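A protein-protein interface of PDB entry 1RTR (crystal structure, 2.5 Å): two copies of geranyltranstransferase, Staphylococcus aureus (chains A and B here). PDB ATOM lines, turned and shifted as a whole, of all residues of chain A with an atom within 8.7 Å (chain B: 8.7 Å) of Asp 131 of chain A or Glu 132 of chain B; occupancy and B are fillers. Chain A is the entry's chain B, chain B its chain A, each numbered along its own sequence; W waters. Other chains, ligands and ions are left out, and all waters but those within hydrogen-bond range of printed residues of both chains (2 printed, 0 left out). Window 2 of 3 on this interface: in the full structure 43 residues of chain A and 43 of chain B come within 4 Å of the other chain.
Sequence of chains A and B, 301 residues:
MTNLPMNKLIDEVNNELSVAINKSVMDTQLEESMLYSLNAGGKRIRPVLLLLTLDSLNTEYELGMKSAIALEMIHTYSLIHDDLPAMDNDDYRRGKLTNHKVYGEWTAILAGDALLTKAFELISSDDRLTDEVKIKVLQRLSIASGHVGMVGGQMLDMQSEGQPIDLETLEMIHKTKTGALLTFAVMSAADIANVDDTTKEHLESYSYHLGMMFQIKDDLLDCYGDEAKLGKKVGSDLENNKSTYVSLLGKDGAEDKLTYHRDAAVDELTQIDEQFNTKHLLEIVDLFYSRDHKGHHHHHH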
ATOM      1  N   ILE A 123      -9.751  11.285  -1.218  1.00  0.00           N
ATOM      2  CA  ILE A 123      -8.347  11.013  -0.903  1.00  0.00           C
ATOM      3  C   ILE A 123      -7.514  10.780  -2.164  1.00  0.00           C
ATOM      4  O   ILE A 123      -6.359  11.210  -2.240  1.00  0.00           O
ATOM      5  CB  ILE A 123      -8.220   9.845   0.097  1.00  0.00           C
ATOM      6  CG1 ILE A 123      -8.780  10.254   1.456  1.00  0.00           C
ATOM      7  CG2 ILE A 123      -6.764   9.412   0.259  1.00  0.00           C
ATOM      8  CD1 ILE A 123      -9.367   9.111   2.228  1.00  0.00           C
ATOM      9  N   SER A 124      -8.111  10.095  -3.138  1.00  0.00           N
ATOM     10  CA  SER A 124      -7.526   9.908  -4.472  1.00  0.00           C
ATOM     11  C   SER A 124      -7.140  11.215  -5.163  1.00  0.00           C
ATOM     12  O   SER A 124      -6.176  11.255  -5.923  1.00  0.00           O
ATOM     13  CB  SER A 124      -8.539   9.230  -5.380  1.00  0.00           C
ATOM     14  OG  SER A 124      -8.443   7.843  -5.260  1.00  0.00           O
ATOM     15  N   SER A 125      -7.917  12.265  -4.919  1.00  0.00           N
ATOM     16  CA  SER A 125      -7.797  13.511  -5.667  1.00  0.00           C
ATOM     17  C   SER A 125      -6.946  14.579  -4.967  1.00  0.00           C
ATOM     18  O   SER A 125      -6.744  15.668  -5.518  1.00  0.00           O
ATOM     19  CB  SER A 125      -9.196  14.070  -5.963  1.00  0.00           C
ATOM     20  OG  SER A 125      -9.697  14.765  -4.825  1.00  0.00           O
ATOM     21  N   ASP A 126      -6.461  14.269  -3.764  1.00  0.00           N
ATOM     22  CA  ASP A 126      -5.763  15.233  -2.915  1.00  0.00           C
ATOM     23  C   ASP A 126      -4.339  15.525  -3.401  1.00  0.00           C
ATOM     24  O   ASP A 126      -3.436  14.681  -3.264  1.00  0.00           O
ATOM     25  CB  ASP A 126      -5.742  14.718  -1.476  1.00  0.00           C
ATOM     26  CG  ASP A 126      -5.342  15.786  -0.469  1.00  0.00           C
ATOM     27  OD1 ASP A 126      -5.232  15.437   0.730  1.00  0.00           O
ATOM     28  OD2 ASP A 126      -5.121  16.988  -0.762  1.00  0.00           O
ATOM     29  N   ASP A 127      -4.136  16.717  -3.972  1.00  0.00           N
ATOM     30  CA  ASP A 127      -2.822  17.053  -4.555  1.00  0.00           C
ATOM     31  C   ASP A 127      -1.819  17.619  -3.548  1.00  0.00           C
ATOM     32  O   ASP A 127      -0.658  17.828  -3.884  1.00  0.00           O
ATOM     33  CB  ASP A 127      -2.926  17.948  -5.806  1.00  0.00           C
ATOM     34  CG  ASP A 127      -3.980  19.042  -5.676  1.00  0.00           C
ATOM     35  OD1 ASP A 127      -4.795  19.191  -6.629  1.00  0.00           O
ATOM     36  OD2 ASP A 127      -4.068  19.795  -4.670  1.00  0.00           O
ATOM     37  N   ARG A 128      -2.270  17.838  -2.313  1.00  0.00           N
ATOM     38  CA  ARG A 128      -1.373  18.233  -1.227  1.00  0.00           C
ATOM     39  C   ARG A 128      -0.519  17.052  -0.744  1.00  0.00           C
ATOM     40  O   ARG A 128       0.444  17.250  -0.010  1.00  0.00           O
ATOM     41  CB  ARG A 128      -2.135  18.846  -0.037  1.00  0.00           C
ATOM     42  CG  ARG A 128      -3.401  19.635  -0.356  1.00  0.00           C
ATOM     43  CD  ARG A 128      -3.218  21.140  -0.372  1.00  0.00           C
ATOM     44  NE  ARG A 128      -3.849  21.826   0.761  1.00  0.00           N
ATOM     45  CZ  ARG A 128      -3.192  22.608   1.630  1.00  0.00           C
ATOM     46  NH1 ARG A 128      -1.872  22.794   1.523  1.00  0.00           N
ATOM     47  NH2 ARG A 128      -3.853  23.198   2.620  1.00  0.00           N
ATOM     48  N   LEU A 129      -0.873  15.834  -1.157  1.00  0.00           N
ATOM     49  CA  LEU A 129      -0.154  14.613  -0.746  1.00  0.00           C
ATOM     50  C   LEU A 129       0.480  13.907  -1.932  1.00  0.00           C
ATOM     51  O   LEU A 129      -0.109  13.850  -3.007  1.00  0.00           O
ATOM     52  CB  LEU A 129      -1.092  13.615  -0.042  1.00  0.00           C
ATOM     53  CG  LEU A 129      -1.956  14.004   1.157  1.00  0.00           C
ATOM     54  CD1 LEU A 129      -2.950  12.905   1.494  1.00  0.00           C
ATOM     55  CD2 LEU A 129      -1.105  14.348   2.366  1.00  0.00           C
ATOM     56  N   THR A 130       1.662  13.333  -1.737  1.00  0.00           N
ATOM     57  CA  THR A 130       2.266  12.533  -2.797  1.00  0.00           C
ATOM     58  C   THR A 130       1.400  11.310  -3.071  1.00  0.00           C
ATOM     59  O   THR A 130       0.551  10.941  -2.253  1.00  0.00           O
ATOM     60  CB  THR A 130       3.724  12.113  -2.462  1.00  0.00           C
ATOM     61  OG1 THR A 130       3.744  11.317  -1.269  1.00  0.00           O
ATOM     62  CG2 THR A 130       4.596  13.337  -2.127  1.00  0.00           C
ATOM     63  N   ASP A 131       1.590  10.695  -4.230  1.00  0.00           N
ATOM     64  CA  ASP A 131       0.856   9.489  -4.557  1.00  0.00           C
ATOM     65  C   ASP A 131       1.146   8.374  -3.562  1.00  0.00           C
ATOM     66  O   ASP A 131       0.254   7.585  -3.238  1.00  0.00           O
ATOM     67  CB  ASP A 131       1.179   9.032  -5.975  1.00  0.00           C
ATOM     68  CG  ASP A 131       0.560   9.934  -7.030  1.00  0.00           C
ATOM     69  OD1 ASP A 131      -0.501  10.551  -6.751  1.00  0.00           O
ATOM     70  OD2 ASP A 131       1.075  10.086  -8.163  1.00  0.00           O
ATOM     71  N   GLU A 132       2.383   8.330  -3.063  1.00  0.00           N
ATOM     72  CA  GLU A 132       2.788   7.285  -2.125  1.00  0.00           C
ATOM     73  C   GLU A 132       2.033   7.348  -0.783  1.00  0.00           C
ATOM     74  O   GLU A 132       1.606   6.306  -0.262  1.00  0.00           O
ATOM     75  CB  GLU A 132       4.319   7.200  -2.012  1.00  0.00           C
ATOM     76  CG  GLU A 132       4.935   7.538  -0.667  1.00  0.00           C
ATOM     77  CD  GLU A 132       6.061   6.586  -0.290  1.00  0.00           C
ATOM     78  OE1 GLU A 132       7.225   6.828  -0.693  1.00  0.00           O
ATOM     79  OE2 GLU A 132       5.777   5.586   0.406  1.00  0.00           O
ATOM     80  N   VAL A 133       1.800   8.554  -0.259  1.00  0.00           N
ATOM     81  CA  VAL A 133       1.032   8.657   0.976  1.00  0.00           C
ATOM     82  C   VAL A 133      -0.466   8.466   0.767  1.00  0.00           C
ATOM     83  O   VAL A 133      -1.128   7.875   1.625  1.00  0.00           O
ATOM     84  CB  VAL A 133       1.400   9.885   1.902  1.00  0.00           C
ATOM     85  CG1 VAL A 133       2.727  10.521   1.524  1.00  0.00           C
ATOM     86  CG2 VAL A 133       0.266  10.914   2.034  1.00  0.00           C
ATOM     87  N   LYS A 134      -0.994   8.936  -0.368  1.00  0.00           N
ATOM     88  CA  LYS A 134      -2.408   8.715  -0.692  1.00  0.00           C
ATOM     89  C   LYS A 134      -2.691   7.221  -0.627  1.00  0.00           C
ATOM     90  O   LYS A 134      -3.681   6.793  -0.037  1.00  0.00           O
ATOM     91  CB  LYS A 134      -2.777   9.246  -2.082  1.00  0.00           C
ATOM     92  CG  LYS A 134      -2.643  10.753  -2.254  1.00  0.00           C
ATOM     93  CD  LYS A 134      -3.676  11.302  -3.233  1.00  0.00           C
ATOM     94  CE  LYS A 134      -3.124  11.438  -4.646  1.00  0.00           C
ATOM     95  NZ  LYS A 134      -2.334  12.691  -4.775  1.00  0.00           N
ATOM     96  N   ILE A 135      -1.812   6.427  -1.218  1.00  0.00           N
ATOM     97  CA  ILE A 135      -1.998   4.983  -1.220  1.00  0.00           C
ATOM     98  C   ILE A 135      -1.967   4.406   0.196  1.00  0.00           C
ATOM     99  O   ILE A 135      -2.795   3.557   0.535  1.00  0.00           O
ATOM    100  CB  ILE A 135      -0.991   4.311  -2.163  1.00  0.00           C
ATOM    101  CG1 ILE A 135      -1.359   4.618  -3.624  1.00  0.00           C
ATOM    102  CG2 ILE A 135      -0.892   2.812  -1.895  1.00  0.00           C
ATOM    103  CD1 ILE A 135      -2.755   4.128  -4.070  1.00  0.00           C
ATOM    104  N   LYS A 136      -1.060   4.919   1.026  1.00  0.00           N
ATOM    105  CA  LYS A 136      -0.950   4.515   2.433  1.00  0.00           C
ATOM    106  C   LYS A 136      -2.217   4.824   3.223  1.00  0.00           C
ATOM    107  O   LYS A 136      -2.709   3.967   3.974  1.00  0.00           O
ATOM    108  CB  LYS A 136       0.246   5.197   3.098  1.00  0.00           C
ATOM    109  CG  LYS A 136       1.585   4.510   2.857  1.00  0.00           C
ATOM    110  CD  LYS A 136       2.698   5.355   3.469  1.00  0.00           C
ATOM    111  CE  LYS A 136       4.073   4.867   3.075  1.00  0.00           C
ATOM    112  NZ  LYS A 136       5.033   6.018   3.060  1.00  0.00           N
ATOM    113  N   VAL A 137      -2.733   6.043   3.048  1.00  0.00           N
ATOM    114  CA  VAL A 137      -3.950   6.490   3.704  1.00  0.00           C
ATOM    115  C   VAL A 137      -5.158   5.700   3.197  1.00  0.00           C
ATOM    116  O   VAL A 137      -5.984   5.218   3.986  1.00  0.00           O
ATOM    117  CB  VAL A 137      -4.160   8.012   3.489  1.00  0.00           C
ATOM    118  CG1 VAL A 137      -5.551   8.455   3.924  1.00  0.00           C
ATOM    119  CG2 VAL A 137      -3.095   8.803   4.225  1.00  0.00           C
ATOM    120  N   LEU A 138      -5.240   5.579   1.872  1.00  0.00           N
ATOM    121  CA  LEU A 138      -6.317   4.875   1.176  1.00  0.00           C
ATOM    122  C   LEU A 138      -6.363   3.400   1.559  1.00  0.00           C
ATOM    123  O   LEU A 138      -7.429   2.842   1.807  1.00  0.00           O
ATOM    124  CB  LEU A 138      -6.083   4.984  -0.323  1.00  0.00           C
ATOM    125  CG  LEU A 138      -7.011   5.527  -1.405  1.00  0.00           C
ATOM    126  CD1 LEU A 138      -8.178   6.324  -0.903  1.00  0.00           C
ATOM    127  CD2 LEU A 138      -6.135   6.357  -2.354  1.00  0.00           C
ATOM    128  N   ILE B 123      -7.118  -2.566  -5.196  1.00  0.00           N
ATOM    129  CA  ILE B 123      -6.330  -1.780  -6.143  1.00  0.00           C
ATOM    130  C   ILE B 123      -5.184  -1.117  -5.407  1.00  0.00           C
ATOM    131  O   ILE B 123      -4.042  -1.142  -5.881  1.00  0.00           O
ATOM    132  CB  ILE B 123      -7.195  -0.732  -6.909  1.00  0.00           C
ATOM    133  CG1 ILE B 123      -8.053  -1.422  -7.964  1.00  0.00           C
ATOM    134  CG2 ILE B 123      -6.311   0.353  -7.558  1.00  0.00           C
ATOM    135  CD1 ILE B 123      -9.326  -0.716  -8.254  1.00  0.00           C
ATOM    136  N   SER B 124      -5.496  -0.542  -4.247  1.00  0.00           N
ATOM    137  CA  SER B 124      -4.505   0.189  -3.460  1.00  0.00           C
ATOM    138  C   SER B 124      -3.364  -0.710  -2.966  1.00  0.00           C
ATOM    139  O   SER B 124      -2.279  -0.216  -2.647  1.00  0.00           O
ATOM    140  CB  SER B 124      -5.167   0.926  -2.295  1.00  0.00           C
ATOM    141  OG  SER B 124      -5.628   0.024  -1.311  1.00  0.00           O
ATOM    142  N   LEU B 129       1.526  -2.513  -9.930  1.00  0.00           N
ATOM    143  CA  LEU B 129       1.361  -1.147 -10.412  1.00  0.00           C
ATOM    144  C   LEU B 129       2.056  -0.160  -9.496  1.00  0.00           C
ATOM    145  O   LEU B 129       2.124  -0.363  -8.291  1.00  0.00           O
ATOM    146  CB  LEU B 129      -0.126  -0.774 -10.515  1.00  0.00           C
ATOM    147  CG  LEU B 129      -1.189  -1.798 -10.935  1.00  0.00           C
ATOM    148  CD1 LEU B 129      -2.577  -1.217 -10.747  1.00  0.00           C
ATOM    149  CD2 LEU B 129      -0.998  -2.261 -12.378  1.00  0.00           C
ATOM    150  N   THR B 130       2.565   0.917 -10.081  1.00  0.00           N
ATOM    151  CA  THR B 130       3.154   2.015  -9.320  1.00  0.00           C
ATOM    152  C   THR B 130       2.055   2.730  -8.560  1.00  0.00           C
ATOM    153  O   THR B 130       0.865   2.564  -8.857  1.00  0.00           O
ATOM    154  CB  THR B 130       3.870   3.034 -10.260  1.00  0.00           C
ATOM    155  OG1 THR B 130       2.898   3.687 -11.099  1.00  0.00           O
ATOM    156  CG2 THR B 130       4.824   2.319 -11.248  1.00  0.00           C
ATOM    157  N   ASP B 131       2.450   3.543  -7.591  1.00  0.00           N
ATOM    158  CA  ASP B 131       1.490   4.339  -6.846  1.00  0.00           C
ATOM    159  C   ASP B 131       0.787   5.362  -7.747  1.00  0.00           C
ATOM    160  O   ASP B 131      -0.413   5.638  -7.577  1.00  0.00           O
ATOM    161  CB  ASP B 131       2.162   4.969  -5.620  1.00  0.00           C
ATOM    162  CG  ASP B 131       2.536   3.922  -4.561  1.00  0.00           C
ATOM    163  OD1 ASP B 131       3.276   4.272  -3.606  1.00  0.00           O
ATOM    164  OD2 ASP B 131       2.134   2.727  -4.607  1.00  0.00           O
ATOM    165  N   GLU B 132       1.521   5.892  -8.723  1.00  0.00           N
ATOM    166  CA  GLU B 132       0.947   6.822  -9.686  1.00  0.00           C
ATOM    167  C   GLU B 132      -0.214   6.175 -10.484  1.00  0.00           C
ATOM    168  O   GLU B 132      -1.295   6.755 -10.589  1.00  0.00           O
ATOM    169  CB  GLU B 132       2.045   7.420 -10.588  1.00  0.00           C
ATOM    170  CG  GLU B 132       1.650   7.654 -12.041  1.00  0.00           C
ATOM    171  CD  GLU B 132       2.007   9.040 -12.534  1.00  0.00           C
ATOM    172  OE1 GLU B 132       3.008   9.166 -13.278  1.00  0.00           O
ATOM    173  OE2 GLU B 132       1.277  10.003 -12.178  1.00  0.00           O
ATOM    174  N   VAL B 133      -0.010   4.969 -11.004  1.00  0.00           N
ATOM    175  CA  VAL B 133      -1.049   4.302 -11.781  1.00  0.00           C
ATOM    176  C   VAL B 133      -2.204   3.884 -10.859  1.00  0.00           C
ATOM    177  O   VAL B 133      -3.375   3.944 -11.243  1.00  0.00           O
ATOM    178  CB  VAL B 133      -0.478   3.097 -12.600  1.00  0.00           C
ATOM    179  CG1 VAL B 133      -1.556   2.368 -13.351  1.00  0.00           C
ATOM    180  CG2 VAL B 133       0.584   3.565 -13.577  1.00  0.00           C
ATOM    181  N   LYS B 134      -1.868   3.483  -9.635  1.00  0.00           N
ATOM    182  CA  LYS B 134      -2.873   3.064  -8.659  1.00  0.00           C
ATOM    183  C   LYS B 134      -3.863   4.180  -8.349  1.00  0.00           C
ATOM    184  O   LYS B 134      -5.070   3.945  -8.282  1.00  0.00           O
ATOM    185  CB  LYS B 134      -2.201   2.612  -7.364  1.00  0.00           C
ATOM    186  CG  LYS B 134      -1.741   1.173  -7.360  1.00  0.00           C
ATOM    187  CD  LYS B 134      -1.351   0.771  -5.958  1.00  0.00           C
ATOM    188  CE  LYS B 134       0.139   0.573  -5.833  1.00  0.00           C
ATOM    189  NZ  LYS B 134       0.345  -0.510  -4.868  1.00  0.00           N
ATOM    190  N   ILE B 135      -3.349   5.392  -8.160  1.00  0.00           N
ATOM    191  CA  ILE B 135      -4.202   6.554  -7.944  1.00  0.00           C
ATOM    192  C   ILE B 135      -5.145   6.772  -9.131  1.00  0.00           C
ATOM    193  O   ILE B 135      -6.340   6.950  -8.942  1.00  0.00           O
ATOM    194  CB  ILE B 135      -3.347   7.817  -7.613  1.00  0.00           C
ATOM    195  CG1 ILE B 135      -2.676   7.671  -6.239  1.00  0.00           C
ATOM    196  CG2 ILE B 135      -4.180   9.082  -7.635  1.00  0.00           C
ATOM    197  CD1 ILE B 135      -3.617   7.282  -5.092  1.00  0.00           C
ATOM    198  N   LYS B 136      -4.611   6.697 -10.350  1.00  0.00           N
ATOM    199  CA  LYS B 136      -5.401   6.909 -11.559  1.00  0.00           C
ATOM    200  C   LYS B 136      -6.583   5.954 -11.648  1.00  0.00           C
ATOM    201  O   LYS B 136      -7.718   6.390 -11.901  1.00  0.00           O
ATOM    202  CB  LYS B 136      -4.532   6.777 -12.797  1.00  0.00           C
ATOM    203  CG  LYS B 136      -3.628   7.952 -13.019  1.00  0.00           C
ATOM    204  CD  LYS B 136      -3.008   7.856 -14.393  1.00  0.00           C
ATOM    205  CE  LYS B 136      -1.662   8.551 -14.442  1.00  0.00           C
ATOM    206  NZ  LYS B 136      -1.081   8.403 -15.802  1.00  0.00           N
ATOM    207  N   VAL B 137      -6.313   4.662 -11.424  1.00  0.00           N
ATOM    208  CA  VAL B 137      -7.350   3.640 -11.411  1.00  0.00           C
ATOM    209  C   VAL B 137      -8.389   3.907 -10.315  1.00  0.00           C
ATOM    210  O   VAL B 137      -9.599   3.869 -10.576  1.00  0.00           O
ATOM    211  CB  VAL B 137      -6.748   2.219 -11.268  1.00  0.00           C
ATOM    212  CG1 VAL B 137      -7.847   1.163 -11.236  1.00  0.00           C
ATOM    213  CG2 VAL B 137      -5.820   1.926 -12.417  1.00  0.00           C
ATOM    214  N   LEU B 138      -7.917   4.172  -9.096  1.00  0.00           N
ATOM    215  CA  LEU B 138      -8.807   4.402  -7.949  1.00  0.00           C
ATOM    216  C   LEU B 138      -9.700   5.615  -8.179  1.00  0.00           C
ATOM    217  O   LEU B 138     -10.912   5.551  -7.969  1.00  0.00           O
ATOM    218  CB  LEU B 138      -8.002   4.597  -6.659  1.00  0.00           C
ATOM    219  CG  LEU B 138      -7.521   3.333  -5.959  1.00  0.00           C
ATOM    220  CD1 LEU B 138      -6.261   3.617  -5.154  1.00  0.00           C
ATOM    221  CD2 LEU B 138      -8.591   2.740  -5.056  1.00  0.00           C
ATOM    222  N   GLN B 139      -9.086   6.712  -8.619  1.00  0.00           N
ATOM    223  CA  GLN B 139      -9.804   7.932  -8.951  1.00  0.00           C
ATOM    224  C   GLN B 139     -10.901   7.641  -9.950  1.00  0.00           C
ATOM    225  O   GLN B 139     -12.049   8.039  -9.756  1.00  0.00           O
ATOM    226  CB  GLN B 139      -8.853   8.975  -9.532  1.00  0.00           C
ATOM    227  CG  GLN B 139      -9.258  10.398  -9.222  1.00  0.00           C
ATOM    228  CD  GLN B 139      -8.228  11.408  -9.688  1.00  0.00           C
ATOM    229  OE1 GLN B 139      -8.564  12.575  -9.901  1.00  0.00           O
ATOM    230  NE2 GLN B 139      -6.968  10.969  -9.853  1.00  0.00           N
ATOM    231  N   ASP B 191      -4.815   3.298 -18.949  1.00  0.00           N
ATOM    232  CA  ASP B 191      -3.960   3.928 -17.932  1.00  0.00           C
ATOM    233  C   ASP B 191      -2.817   3.023 -17.453  1.00  0.00           C
ATOM    234  O   ASP B 191      -1.680   3.481 -17.269  1.00  0.00           O
ATOM    235  CB  ASP B 191      -4.806   4.417 -16.748  1.00  0.00           C
ATOM    236  CG  ASP B 191      -5.388   5.805 -16.980  1.00  0.00           C
ATOM    237  OD1 ASP B 191      -4.957   6.478 -17.944  1.00  0.00           O
ATOM    238  OD2 ASP B 191      -6.283   6.311 -16.263  1.00  0.00           O
ATOM    239  N   ILE B 192      -3.115   1.739 -17.249  1.00  0.00           N
ATOM    240  CA  ILE B 192      -2.074   0.785 -16.902  1.00  0.00           C
ATOM    241  C   ILE B 192      -1.087   0.652 -18.067  1.00  0.00           C
ATOM    242  O   ILE B 192       0.133   0.611 -17.849  1.00  0.00           O
ATOM    243  CB  ILE B 192      -2.682  -0.559 -16.520  1.00  0.00           C
ATOM    244  CG1 ILE B 192      -3.423  -0.438 -15.188  1.00  0.00           C
ATOM    245  CG2 ILE B 192      -1.597  -1.648 -16.478  1.00  0.00           C
ATOM    246  CD1 ILE B 192      -4.599  -1.379 -15.052  1.00  0.00           C
ATOM    247  N   ASN B 194      -0.403   2.902 -20.209  1.00  0.00           N
ATOM    248  CA  ASN B 194       0.279   4.174 -20.445  1.00  0.00           C
ATOM    249  C   ASN B 194       0.282   4.584 -21.922  1.00  0.00           C
ATOM    250  O   ASN B 194       1.263   5.122 -22.427  1.00  0.00           O
ATOM    251  CB  ASN B 194       1.707   4.122 -19.887  1.00  0.00           C
ATOM    252  CG  ASN B 194       2.383   5.468 -19.887  1.00  0.00           C
ATOM    253  OD1 ASN B 194       3.579   5.569 -20.172  1.00  0.00           O
ATOM    254  ND2 ASN B 194       1.622   6.520 -19.590  1.00  0.00           N
HETATM  255  O   HOH W   1      -1.144   9.255 -10.353  1.00  0.00           O
HETATM  256  O   HOH W   2       2.297   3.996  -0.884  1.00  0.00           O
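The backbone carbonyl oxygen (O) of Ser 124 of chain B lies within hydrogen-bond range of the side-chain amino group (NZ) of Lys 134 of chain B (3.5 Å).
The side-chain amino group (NZ) of Lys 134 of chain B lies within salt-bridge range of the side-chain carboxylate (OD2) of Asp 131 of chain B (3.7 Å).
The side-chain amino group (NZ) of Lys 134 of chain A is in hydrogen-bond range of the backbone carbonyl oxygen (O) of Asp 126 of chain A, 2.7 Å away.
The backbone carbonyl oxygen of Leu 129 of chain A is in hydrogen-bond range of the side-chain amino group of Lys 134 of chain A, 3.1 Å away.
The side-chain carboxylate (OD1) of Asp 131 of chain A lies within salt-bridge range of the side-chain amino group (NZ) of Lys 134 of chain A, at 3.4 Å.
The side-chain carboxylate (OE2) of Glu 132 of chain A is in salt-bridge range of the side-chain amino group (NZ) of Lys 136 of chain A (2.8 Å).
Printed residues of chain A that touch a printed residue of chain B: Ser 124, Asp 131, Glu 132, Lys 134, Ile 135 and Leu 138.
Hydrophobic or aromatic side chains of chain A that line the printed part of chain B: Ile 135 and Leu 138.
Hydrophobic or aromatic side chains of chain B that line the printed part of chain A: Ile 135 and Leu 138.
Among the printed residues, no Asp or Glu carboxylate lies within 4 Å of a Lys or Arg side-chain nitrogen of the other chain.
Ser 124 of chain A touches Leu 138 of chain B, but with the chains exchanged Leu 138 of chain A does not touch Ser 124 of chain B (4.5 Å).
Asp 131 of chain A touches Ile 135 of chain B, but with the chains exchanged Ile 135 of chain A does not touch Asp 131 of chain B (4.1 Å).
Ile 135 of chain A touches Leu 138 of chain B, and with the chains exchanged Leu 138 of chain A touches Ile 135 of chain B.
Leu 138 of chain A touches its own counterpart, Leu 138 of chain B.
Among the printed residues, pairs that only touch across the chains: Glu 132 of chain A with Asp 131 of chain B (3.4 Å), Ser 124 of chain A with Ile 135 of chain B (3.4 Å), Ile 135 of chain A with Ser 124 of chain B (3.4 Å), Ile 135 of chain A with Ile 135 of chain B (3.4 Å), Ser 124 of chain A with Leu 138 of chain B (3.6 Å), Ser 124 of chain A with Gln 139 of chain B (3.6 Å), Asp 131 of chain A with Glu 132 of chain B (3.6 Å), Asp 131 of chain A with Ile 135 of chain B (3.6 Å), Ile 135 of chain A with Lys 134 of chain B (3.7 Å), Lys 134 of chain A with Ile 135 of chain B (3.7 Å), Ile 135 of chain A with Leu 138 of chain B (3.7 Å), Leu 138 of chain A with Ile 135 of chain B (3.8 Å) and Leu 138 of chain A with Leu 138 of chain B (3.9 Å).
Water W2 lies within hydrogen-bond range of O of Glu 132 of chain A (2.5 Å) and OD1 of Asp 131 of chain B (2.9 Å).
Water W1 bridges the backbone carbonyl oxygen of Glu 132 of chain B and the side-chain carboxylate of Asp 131 of chain A.
Printed residues of chain B within 4 Å of Asp 131 of chain A: Glu 132 (3.6 Å) and Ile 135 (3.6 Å).
Glu 132 of chain B touches just one residue of chain A: Asp 131 (3.6 Å).
Printed residues of chain B within 4 Å of Ile 135 of chain A: Ser 124, Lys 134, Ile 135 and Leu 138.
Of the printed residues of chain A, Gln 139 of chain B touches Ser 124.
Printed residues of chain B within 4 Å of Leu 138 of chain A: Ile 135 and Leu 138.
Printed residues of chain B within 4 Å of Glu 132 of chain A: Asp 131.
Arg 128 of chain A touches none of the printed residues of chain B.
Asn 194 of chain B touches none of the printed residues of chain A.
The nearest printed residue of chain B that does not touch Asp 131 of chain A is Asp 131 of chain B (4.02 Å).
The nearest printed residue of chain A that does not touch Ile 135 of chain B is Ile 123 of chain A (5.6 Å).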
